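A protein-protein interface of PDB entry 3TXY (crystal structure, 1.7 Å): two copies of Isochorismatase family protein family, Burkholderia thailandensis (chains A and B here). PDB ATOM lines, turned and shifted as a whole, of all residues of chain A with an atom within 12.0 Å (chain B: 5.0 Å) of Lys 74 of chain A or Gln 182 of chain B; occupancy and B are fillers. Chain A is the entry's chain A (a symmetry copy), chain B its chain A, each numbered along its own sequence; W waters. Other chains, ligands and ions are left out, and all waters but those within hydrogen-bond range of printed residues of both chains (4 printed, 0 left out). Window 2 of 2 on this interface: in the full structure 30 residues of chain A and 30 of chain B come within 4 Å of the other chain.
Of the 12 printed residues of chain A, 5 touch a printed residue of chain B. Hydrophobic or aromatic side chains of chain A that line the printed part of chain B: Val 73 and Trp 109. Of the 12 printed residues of chain B, 5 touch a printed residue of chain A. Hydrophobic or aromatic side chains of chain B within 4 Å of the printed part of chain A: Leu 180 and Val 183. Among the printed residues, no Asp or Glu carboxylate lies within 4 Å of a Lys or Arg side-chain nitrogen of the other chain.
Lys 74 of chain A touches three residues of chain B. Printed residues of chain A within 4 Å of Gln 182 of chain B: Lys 74 and Asp 76. No residue of chain A comes within 4 Å of Pro 8 of chain B. Asn 153 of chain B touches just these residues of chain A: Val 73 (3.3 Å) and Lys 74 (2.9 Å). Val 183 of chain B touches one residue of chain A. No residue of chain A comes within 4 Å of Ala 184 of chain B. Of the printed residues of chain A, Leu 180 of chain B touches Thr 75 (3.6 Å) and Trp 109 (3.7 Å). Of the printed residues of chain B, Thr 75 of chain A touches Leu 180 and Gly 181. Of the printed residues of chain B, Asp 76 of chain A touches Gly 181, Gln 182 and Val 183. Of the printed residues of chain B, Trp 109 of chain A touches Leu 180. The nearest residue of chain B that does not touch Lys 74 of chain A is Thr 9 of chain B (4.2 Å). The nearest printed residue of chain A that does not touch Leu 180 of chain B is Lys 74 of chain A (4.5 Å).
N of Val 183 of chain B lies within hydrogen-bond range of OD2 of Asp 76 of chain A, at 2.9 Å. O of Gly 181 of chain B lies within hydrogen-bond range of N of Asp 76 of chain A (2.8 Å). The side-chain amide oxygen of Asn 153 of chain B lies within hydrogen-bond range of the backbone NH of Lys 74 of chain A, at 2.9 Å.
O of Gln 182 of chain B sits at hydrogen-bond distance from N of Val 156 of chain B (2.8 Å). The backbone carbonyl oxygen (O) of Val 154 of chain B is in hydrogen-bond range of the backbone NH (N) of Gln 182 of chain B, 2.9 Å away. The side-chain amide nitrogen (NE2) of Gln 182 of chain B sits at hydrogen-bond distance from the backbone carbonyl oxygen (O) of Thr 9 of chain B, at 2.9 Å. The side-chain hydroxyl of Thr 75 of chain A is in hydrogen-bond range of the backbone carbonyl oxygen of Val 77 of chain A (2.7 Å).
Among the printed residues, pairs that only touch across the chains: Val 73 of chain A with Asn 153 of chain B, Lys 74 of chain A with Gly 181 of chain B, Lys 74 of chain A with Gln 182 of chain B, Thr 75 of chain A with Leu 180 of chain B, Thr 75 of chain A with Gly 181 of chain B, Asp 76 of chain A with Gln 182 of chain B and Trp 109 of chain A with Leu 180 of chain B.
No position is printed for both chains. Of the 10 pairs that touch across the chains among the printed residues, none has its exchanged pair printed and touching as well.
Water W4 lies within hydrogen-bond range of the backbone carbonyl oxygen (O) of Val 183 of chain B (2.6 Å) and the side-chain carboxylate (OD1) of Asp 76 of chain A (2.8 Å). Water W1 lies within hydrogen-bond range of the side-chain amide oxygen of Gln 182 of chain B (2.7 Å) and the side-chain carboxylate of Asp 76 of chain A (3.0 Å). Water W3 lies within hydrogen-bond range of O of Leu 180 of chain B (2.7 Å), N of Val 154 of chain B (2.9 Å) and O of Lys 74 of chain A (3.3 Å). Water W2 lies within hydrogen-bond range of O of Lys 74 of chain A (2.7 Å), O of Val 154 of chain B (2.9 Å) and NE2 of Gln 182 of chain B (2.9 Å).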
ATOM      1  N   ALA A  70     -12.565  14.842 -20.602  1.00  0.00           N
ATOM      2  CA  ALA A  70     -12.235  15.733 -19.487  1.00  0.00           C
ATOM      3  C   ALA A  70     -12.115  17.149 -20.001  1.00  0.00           C
ATOM      4  O   ALA A  70     -11.503  17.369 -21.056  1.00  0.00           O
ATOM      5  CB  ALA A  70     -10.906  15.335 -18.850  1.00  0.00           C
ATOM      6  N   LEU A  71     -12.645  18.119 -19.259  1.00  0.00           N
ATOM      7  CA  LEU A  71     -12.526  19.528 -19.688  1.00  0.00           C
ATOM      8  C   LEU A  71     -11.071  19.945 -19.669  1.00  0.00           C
ATOM      9  O   LEU A  71     -10.306  19.568 -18.744  1.00  0.00           O
ATOM     10  CB  LEU A  71     -13.353  20.468 -18.797  1.00  0.00           C
ATOM     11  CG  LEU A  71     -14.864  20.371 -19.038  1.00  0.00           C
ATOM     12  CD1 LEU A  71     -15.653  20.849 -17.817  1.00  0.00           C
ATOM     13  CD2 LEU A  71     -15.259  21.160 -20.274  1.00  0.00           C
ATOM     14  N   LYS A  72     -10.665  20.647 -20.732  1.00  0.00           N
ATOM     15  CA  LYS A  72      -9.302  21.154 -20.880  1.00  0.00           C
ATOM     16  C   LYS A  72      -9.299  22.691 -21.027  1.00  0.00           C
ATOM     17  O   LYS A  72      -8.280  23.296 -21.386  1.00  0.00           O
ATOM     18  CB  LYS A  72      -8.609  20.458 -22.078  1.00  0.00           C
ATOM     19  N   VAL A  73     -10.422  23.318 -20.682  1.00  0.00           N
ATOM     20  CA  VAL A  73     -10.518  24.768 -20.655  1.00  0.00           C
ATOM     21  C   VAL A  73      -9.481  25.361 -19.691  1.00  0.00           C
ATOM     22  O   VAL A  73      -9.045  24.713 -18.724  1.00  0.00           O
ATOM     23  CB  VAL A  73     -11.941  25.249 -20.257  1.00  0.00           C
ATOM     24  CG1 VAL A  73     -12.934  24.839 -21.328  1.00  0.00           C
ATOM     25  CG2 VAL A  73     -12.354  24.702 -18.891  1.00  0.00           C
ATOM     26  N   LYS A  74      -9.129  26.613 -19.958  1.00  0.00           N
ATOM     27  CA  LYS A  74      -8.081  27.311 -19.222  1.00  0.00           C
ATOM     28  C   LYS A  74      -8.594  27.726 -17.835  1.00  0.00           C
ATOM     29  O   LYS A  74      -9.621  28.395 -17.708  1.00  0.00           O
ATOM     30  CB  LYS A  74      -7.569  28.506 -20.043  1.00  0.00           C
ATOM     31  CG  LYS A  74      -6.567  29.399 -19.320  1.00  0.00           C
ATOM     32  CD  LYS A  74      -5.220  28.750 -19.086  1.00  0.00           C
ATOM     33  CE  LYS A  74      -4.379  29.605 -18.152  1.00  0.00           C
ATOM     34  NZ  LYS A  74      -3.056  28.975 -17.916  1.00  0.00           N
ATOM     35  N   THR A  75      -7.895  27.260 -16.800  1.00  0.00           N
ATOM     36  CA  THR A  75      -8.218  27.586 -15.416  1.00  0.00           C
ATOM     37  C   THR A  75      -6.948  28.051 -14.697  1.00  0.00           C
ATOM     38  O   THR A  75      -5.839  27.655 -15.061  1.00  0.00           O
ATOM     39  CB  THR A  75      -8.866  26.384 -14.657  1.00  0.00           C
ATOM     40  OG1 THR A  75      -7.914  25.329 -14.457  1.00  0.00           O
ATOM     41  CG2 THR A  75     -10.074  25.831 -15.410  1.00  0.00           C
ATOM     42  N   ASP A  76      -7.111  28.909 -13.694  1.00  0.00           N
ATOM     43  CA  ASP A  76      -5.985  29.399 -12.898  1.00  0.00           C
ATOM     44  C   ASP A  76      -5.335  28.284 -12.096  1.00  0.00           C
ATOM     45  O   ASP A  76      -4.120  28.277 -11.932  1.00  0.00           O
ATOM     46  CB  ASP A  76      -6.431  30.511 -11.943  1.00  0.00           C
ATOM     47  CG  ASP A  76      -6.671  31.843 -12.646  1.00  0.00           C
ATOM     48  OD1 ASP A  76      -6.093  32.074 -13.738  1.00  0.00           O
ATOM     49  OD2 ASP A  76      -7.418  32.676 -12.082  1.00  0.00           O
ATOM     50  N   VAL A  77      -6.147  27.369 -11.587  1.00  0.00           N
ATOM     51  CA  VAL A  77      -5.654  26.212 -10.854  1.00  0.00           C
ATOM     52  C   VAL A  77      -5.651  25.031 -11.803  1.00  0.00           C
ATOM     53  O   VAL A  77      -6.723  24.534 -12.145  1.00  0.00           O
ATOM     54  CB  VAL A  77      -6.561  25.862  -9.659  1.00  0.00           C
ATOM     55  CG1 VAL A  77      -6.187  24.500  -9.074  1.00  0.00           C
ATOM     56  CG2 VAL A  77      -6.473  26.945  -8.598  1.00  0.00           C
ATOM     57  N   PRO A  78      -4.457  24.557 -12.205  1.00  0.00           N
ATOM     58  CA  PRO A  78      -4.436  23.409 -13.116  1.00  0.00           C
ATOM     59  C   PRO A  78      -5.152  22.212 -12.497  1.00  0.00           C
ATOM     60  O   PRO A  78      -4.901  21.891 -11.335  1.00  0.00           O
ATOM     61  CB  PRO A  78      -2.945  23.118 -13.272  1.00  0.00           C
ATOM     62  CG  PRO A  78      -2.332  23.588 -11.997  1.00  0.00           C
ATOM     63  CD  PRO A  78      -3.132  24.802 -11.605  1.00  0.00           C
ATOM     64  N   PRO A  79      -6.070  21.574 -13.249  1.00  0.00           N
ATOM     65  CA  PRO A  79      -6.706  20.366 -12.718  1.00  0.00           C
ATOM     66  C   PRO A  79      -5.762  19.154 -12.730  1.00  0.00           C
ATOM     67  O   PRO A  79      -4.773  19.136 -13.478  1.00  0.00           O
ATOM     68  CB  PRO A  79      -7.881  20.122 -13.669  1.00  0.00           C
ATOM     69  CG  PRO A  79      -7.609  20.932 -14.898  1.00  0.00           C
ATOM     70  CD  PRO A  79      -6.428  21.831 -14.656  1.00  0.00           C
ATOM     71  N   SER A  80      -6.076  18.158 -11.903  1.00  0.00           N
ATOM     72  CA  SER A  80      -5.416  16.855 -11.993  1.00  0.00           C
ATOM     73  C   SER A  80      -5.670  16.281 -13.387  1.00  0.00           C
ATOM     74  O   SER A  80      -6.757  16.481 -13.948  1.00  0.00           O
ATOM     75  CB  SER A  80      -5.966  15.884 -10.948  1.00  0.00           C
ATOM     76  OG  SER A  80      -5.710  16.338  -9.628  1.00  0.00           O
ATOM     77  N   TRP A 109     -18.291  18.621 -13.148  1.00  0.00           N
ATOM     78  CA  TRP A 109     -18.763  18.821 -11.775  1.00  0.00           C
ATOM     79  C   TRP A 109     -20.180  18.395 -11.581  1.00  0.00           C
ATOM     80  O   TRP A 109     -20.452  17.434 -10.845  1.00  0.00           O
ATOM     81  CB  TRP A 109     -18.629  20.271 -11.338  1.00  0.00           C
ATOM     82  CG  TRP A 109     -17.221  20.794 -11.233  1.00  0.00           C
ATOM     83  CD1 TRP A 109     -16.030  20.156 -11.557  1.00  0.00           C
ATOM     84  CD2 TRP A 109     -16.833  22.154 -10.856  1.00  0.00           C
ATOM     85  NE1 TRP A 109     -14.959  20.996 -11.356  1.00  0.00           N
ATOM     86  CE2 TRP A 109     -15.375  22.211 -10.949  1.00  0.00           C
ATOM     87  CE3 TRP A 109     -17.523  23.274 -10.447  1.00  0.00           C
ATOM     88  CZ2 TRP A 109     -14.668  23.357 -10.633  1.00  0.00           C
ATOM     89  CZ3 TRP A 109     -16.807  24.423 -10.139  1.00  0.00           C
ATOM     90  CH2 TRP A 109     -15.412  24.461 -10.221  1.00  0.00           C
ATOM     91  N   PRO B   8      -4.856  37.455 -18.228  1.00  0.00           N
ATOM     92  CA  PRO B   8      -5.442  36.171 -18.584  1.00  0.00           C
ATOM     93  C   PRO B   8      -5.098  35.776 -20.008  1.00  0.00           C
ATOM     94  O   PRO B   8      -4.775  36.633 -20.837  1.00  0.00           O
ATOM     95  CB  PRO B   8      -6.944  36.439 -18.460  1.00  0.00           C
ATOM     96  CG  PRO B   8      -7.080  37.888 -18.765  1.00  0.00           C
ATOM     97  CD  PRO B   8      -5.874  38.511 -18.128  1.00  0.00           C
ATOM     98  N   THR B   9      -5.154  34.483 -20.282  1.00  0.00           N
ATOM     99  CA  THR B   9      -5.012  33.988 -21.633  1.00  0.00           C
ATOM    100  C   THR B   9      -6.375  33.995 -22.305  1.00  0.00           C
ATOM    101  O   THR B   9      -7.335  33.407 -21.771  1.00  0.00           O
ATOM    102  CB  THR B   9      -4.494  32.547 -21.657  1.00  0.00           C
ATOM    103  OG1 THR B   9      -3.229  32.476 -20.986  1.00  0.00           O
ATOM    104  CG2 THR B   9      -4.340  32.083 -23.094  1.00  0.00           C
ATOM    105  N   ASN B 153     -13.987  28.736 -22.231  1.00  0.00           N
ATOM    106  CA  ASN B 153     -12.954  29.335 -21.376  1.00  0.00           C
ATOM    107  C   ASN B 153     -13.573  30.556 -20.699  1.00  0.00           C
ATOM    108  O   ASN B 153     -14.014  31.498 -21.378  1.00  0.00           O
ATOM    109  CB  ASN B 153     -11.732  29.735 -22.173  1.00  0.00           C
ATOM    110  CG  ASN B 153     -11.113  28.563 -22.882  1.00  0.00           C
ATOM    111  OD1 ASN B 153     -10.533  27.670 -22.245  1.00  0.00           O
ATOM    112  ND2 ASN B 153     -11.239  28.544 -24.204  1.00  0.00           N
ATOM    113  N   VAL B 154     -13.662  30.508 -19.375  1.00  0.00           N
ATOM    114  CA  VAL B 154     -14.330  31.560 -18.601  1.00  0.00           C
ATOM    115  C   VAL B 154     -13.304  32.450 -17.892  1.00  0.00           C
ATOM    116  O   VAL B 154     -12.382  31.959 -17.236  1.00  0.00           O
ATOM    117  CB  VAL B 154     -15.269  30.974 -17.535  1.00  0.00           C
ATOM    118  CG1 VAL B 154     -15.942  32.088 -16.724  1.00  0.00           C
ATOM    119  CG2 VAL B 154     -16.315  30.037 -18.154  1.00  0.00           C
ATOM    120  N   VAL B 155     -13.491  33.760 -18.021  1.00  0.00           N
ATOM    121  CA  VAL B 155     -12.726  34.745 -17.290  1.00  0.00           C
ATOM    122  C   VAL B 155     -13.722  35.592 -16.503  1.00  0.00           C
ATOM    123  O   VAL B 155     -14.675  36.154 -17.078  1.00  0.00           O
ATOM    124  CB  VAL B 155     -11.902  35.639 -18.242  1.00  0.00           C
ATOM    125  CG1 VAL B 155     -11.080  36.663 -17.453  1.00  0.00           C
ATOM    126  CG2 VAL B 155     -11.014  34.765 -19.122  1.00  0.00           C
ATOM    127  N   VAL B 156     -13.505  35.700 -15.198  1.00  0.00           N
ATOM    128  CA  VAL B 156     -14.323  36.561 -14.344  1.00  0.00           C
ATOM    129  C   VAL B 156     -13.549  37.831 -13.950  1.00  0.00           C
ATOM    130  O   VAL B 156     -12.395  37.767 -13.539  1.00  0.00           O
ATOM    131  CB  VAL B 156     -14.810  35.827 -13.094  1.00  0.00           C
ATOM    132  CG1 VAL B 156     -15.775  36.697 -12.314  1.00  0.00           C
ATOM    133  CG2 VAL B 156     -15.495  34.539 -13.507  1.00  0.00           C
ATOM    134  N   PHE B 177     -13.864  30.196  -8.572  1.00  0.00           N
ATOM    135  CA  PHE B 177     -13.590  30.616  -9.937  1.00  0.00           C
ATOM    136  C   PHE B 177     -12.234  30.145 -10.490  1.00  0.00           C
ATOM    137  O   PHE B 177     -12.159  29.792 -11.663  1.00  0.00           O
ATOM    138  CB  PHE B 177     -13.726  32.120 -10.077  1.00  0.00           C
ATOM    139  CG  PHE B 177     -15.131  32.635  -9.882  1.00  0.00           C
ATOM    140  CD1 PHE B 177     -16.243  31.803  -9.984  1.00  0.00           C
ATOM    141  CD2 PHE B 177     -15.332  33.986  -9.657  1.00  0.00           C
ATOM    142  CE1 PHE B 177     -17.521  32.318  -9.822  1.00  0.00           C
ATOM    143  CE2 PHE B 177     -16.598  34.497  -9.493  1.00  0.00           C
ATOM    144  CZ  PHE B 177     -17.698  33.671  -9.580  1.00  0.00           C
ATOM    145  N   LEU B 180     -12.584  26.813 -12.296  1.00  0.00           N
ATOM    146  CA  LEU B 180     -13.424  26.711 -13.477  1.00  0.00           C
ATOM    147  C   LEU B 180     -13.013  27.732 -14.547  1.00  0.00           C
ATOM    148  O   LEU B 180     -13.563  27.740 -15.639  1.00  0.00           O
ATOM    149  CB  LEU B 180     -14.916  26.812 -13.095  1.00  0.00           C
ATOM    150  CG  LEU B 180     -15.412  28.071 -12.392  1.00  0.00           C
ATOM    151  CD1 LEU B 180     -15.226  29.337 -13.229  1.00  0.00           C
ATOM    152  CD2 LEU B 180     -16.882  27.945 -11.949  1.00  0.00           C
ATOM    153  N   GLY B 181     -12.021  28.563 -14.261  1.00  0.00           N
ATOM    154  CA  GLY B 181     -11.617  29.572 -15.211  1.00  0.00           C
ATOM    155  C   GLY B 181     -10.519  30.446 -14.640  1.00  0.00           C
ATOM    156  O   GLY B 181      -9.742  30.001 -13.776  1.00  0.00           O
ATOM    157  N   GLN B 182     -10.478  31.687 -15.126  1.00  0.00           N
ATOM    158  CA  GLN B 182      -9.438  32.663 -14.769  1.00  0.00           C
ATOM    159  C   GLN B 182     -10.052  33.917 -14.149  1.00  0.00           C
ATOM    160  O   GLN B 182     -11.105  34.363 -14.578  1.00  0.00           O
ATOM    161  CB  GLN B 182      -8.658  33.091 -16.017  1.00  0.00           C
ATOM    162  CG  GLN B 182      -8.035  31.974 -16.822  1.00  0.00           C
ATOM    163  CD  GLN B 182      -7.392  32.502 -18.104  1.00  0.00           C
ATOM    164  OE1 GLN B 182      -6.249  32.985 -18.088  1.00  0.00           O
ATOM    165  NE2 GLN B 182      -8.118  32.413 -19.206  1.00  0.00           N
ATOM    166  N   VAL B 183      -9.386  34.457 -13.138  1.00  0.00           N
ATOM    167  CA  VAL B 183      -9.813  35.679 -12.464  1.00  0.00           C
ATOM    168  C   VAL B 183      -8.819  36.779 -12.810  1.00  0.00           C
ATOM    169  O   VAL B 183      -7.606  36.585 -12.702  1.00  0.00           O
ATOM    170  CB  VAL B 183      -9.925  35.469 -10.946  1.00  0.00           C
ATOM    171  CG1 VAL B 183     -10.429  36.714 -10.240  1.00  0.00           C
ATOM    172  CG2 VAL B 183     -10.870  34.303 -10.635  1.00  0.00           C
ATOM    173  N   ALA B 184      -9.323  37.910 -13.281  1.00  0.00           N
ATOM    174  CA  ALA B 184      -8.457  39.013 -13.702  1.00  0.00           C
ATOM    175  C   ALA B 184      -9.188  40.332 -13.521  1.00  0.00           C
ATOM    176  O   ALA B 184     -10.406  40.346 -13.360  1.00  0.00           O
ATOM    177  CB  ALA B 184      -8.060  38.819 -15.156  1.00  0.00           C
HETATM  178  O   HOH W   1      -4.794  33.646 -15.937  1.00  0.00           O
HETATM  179  O   HOH W   2     -10.471  30.646 -19.003  1.00  0.00           O
HETATM  180  O   HOH W   3     -12.843  28.024 -18.238  1.00  0.00           O
HETATM  181  O   HOH W   4      -6.030  34.855 -13.921  1.00  0.00           O
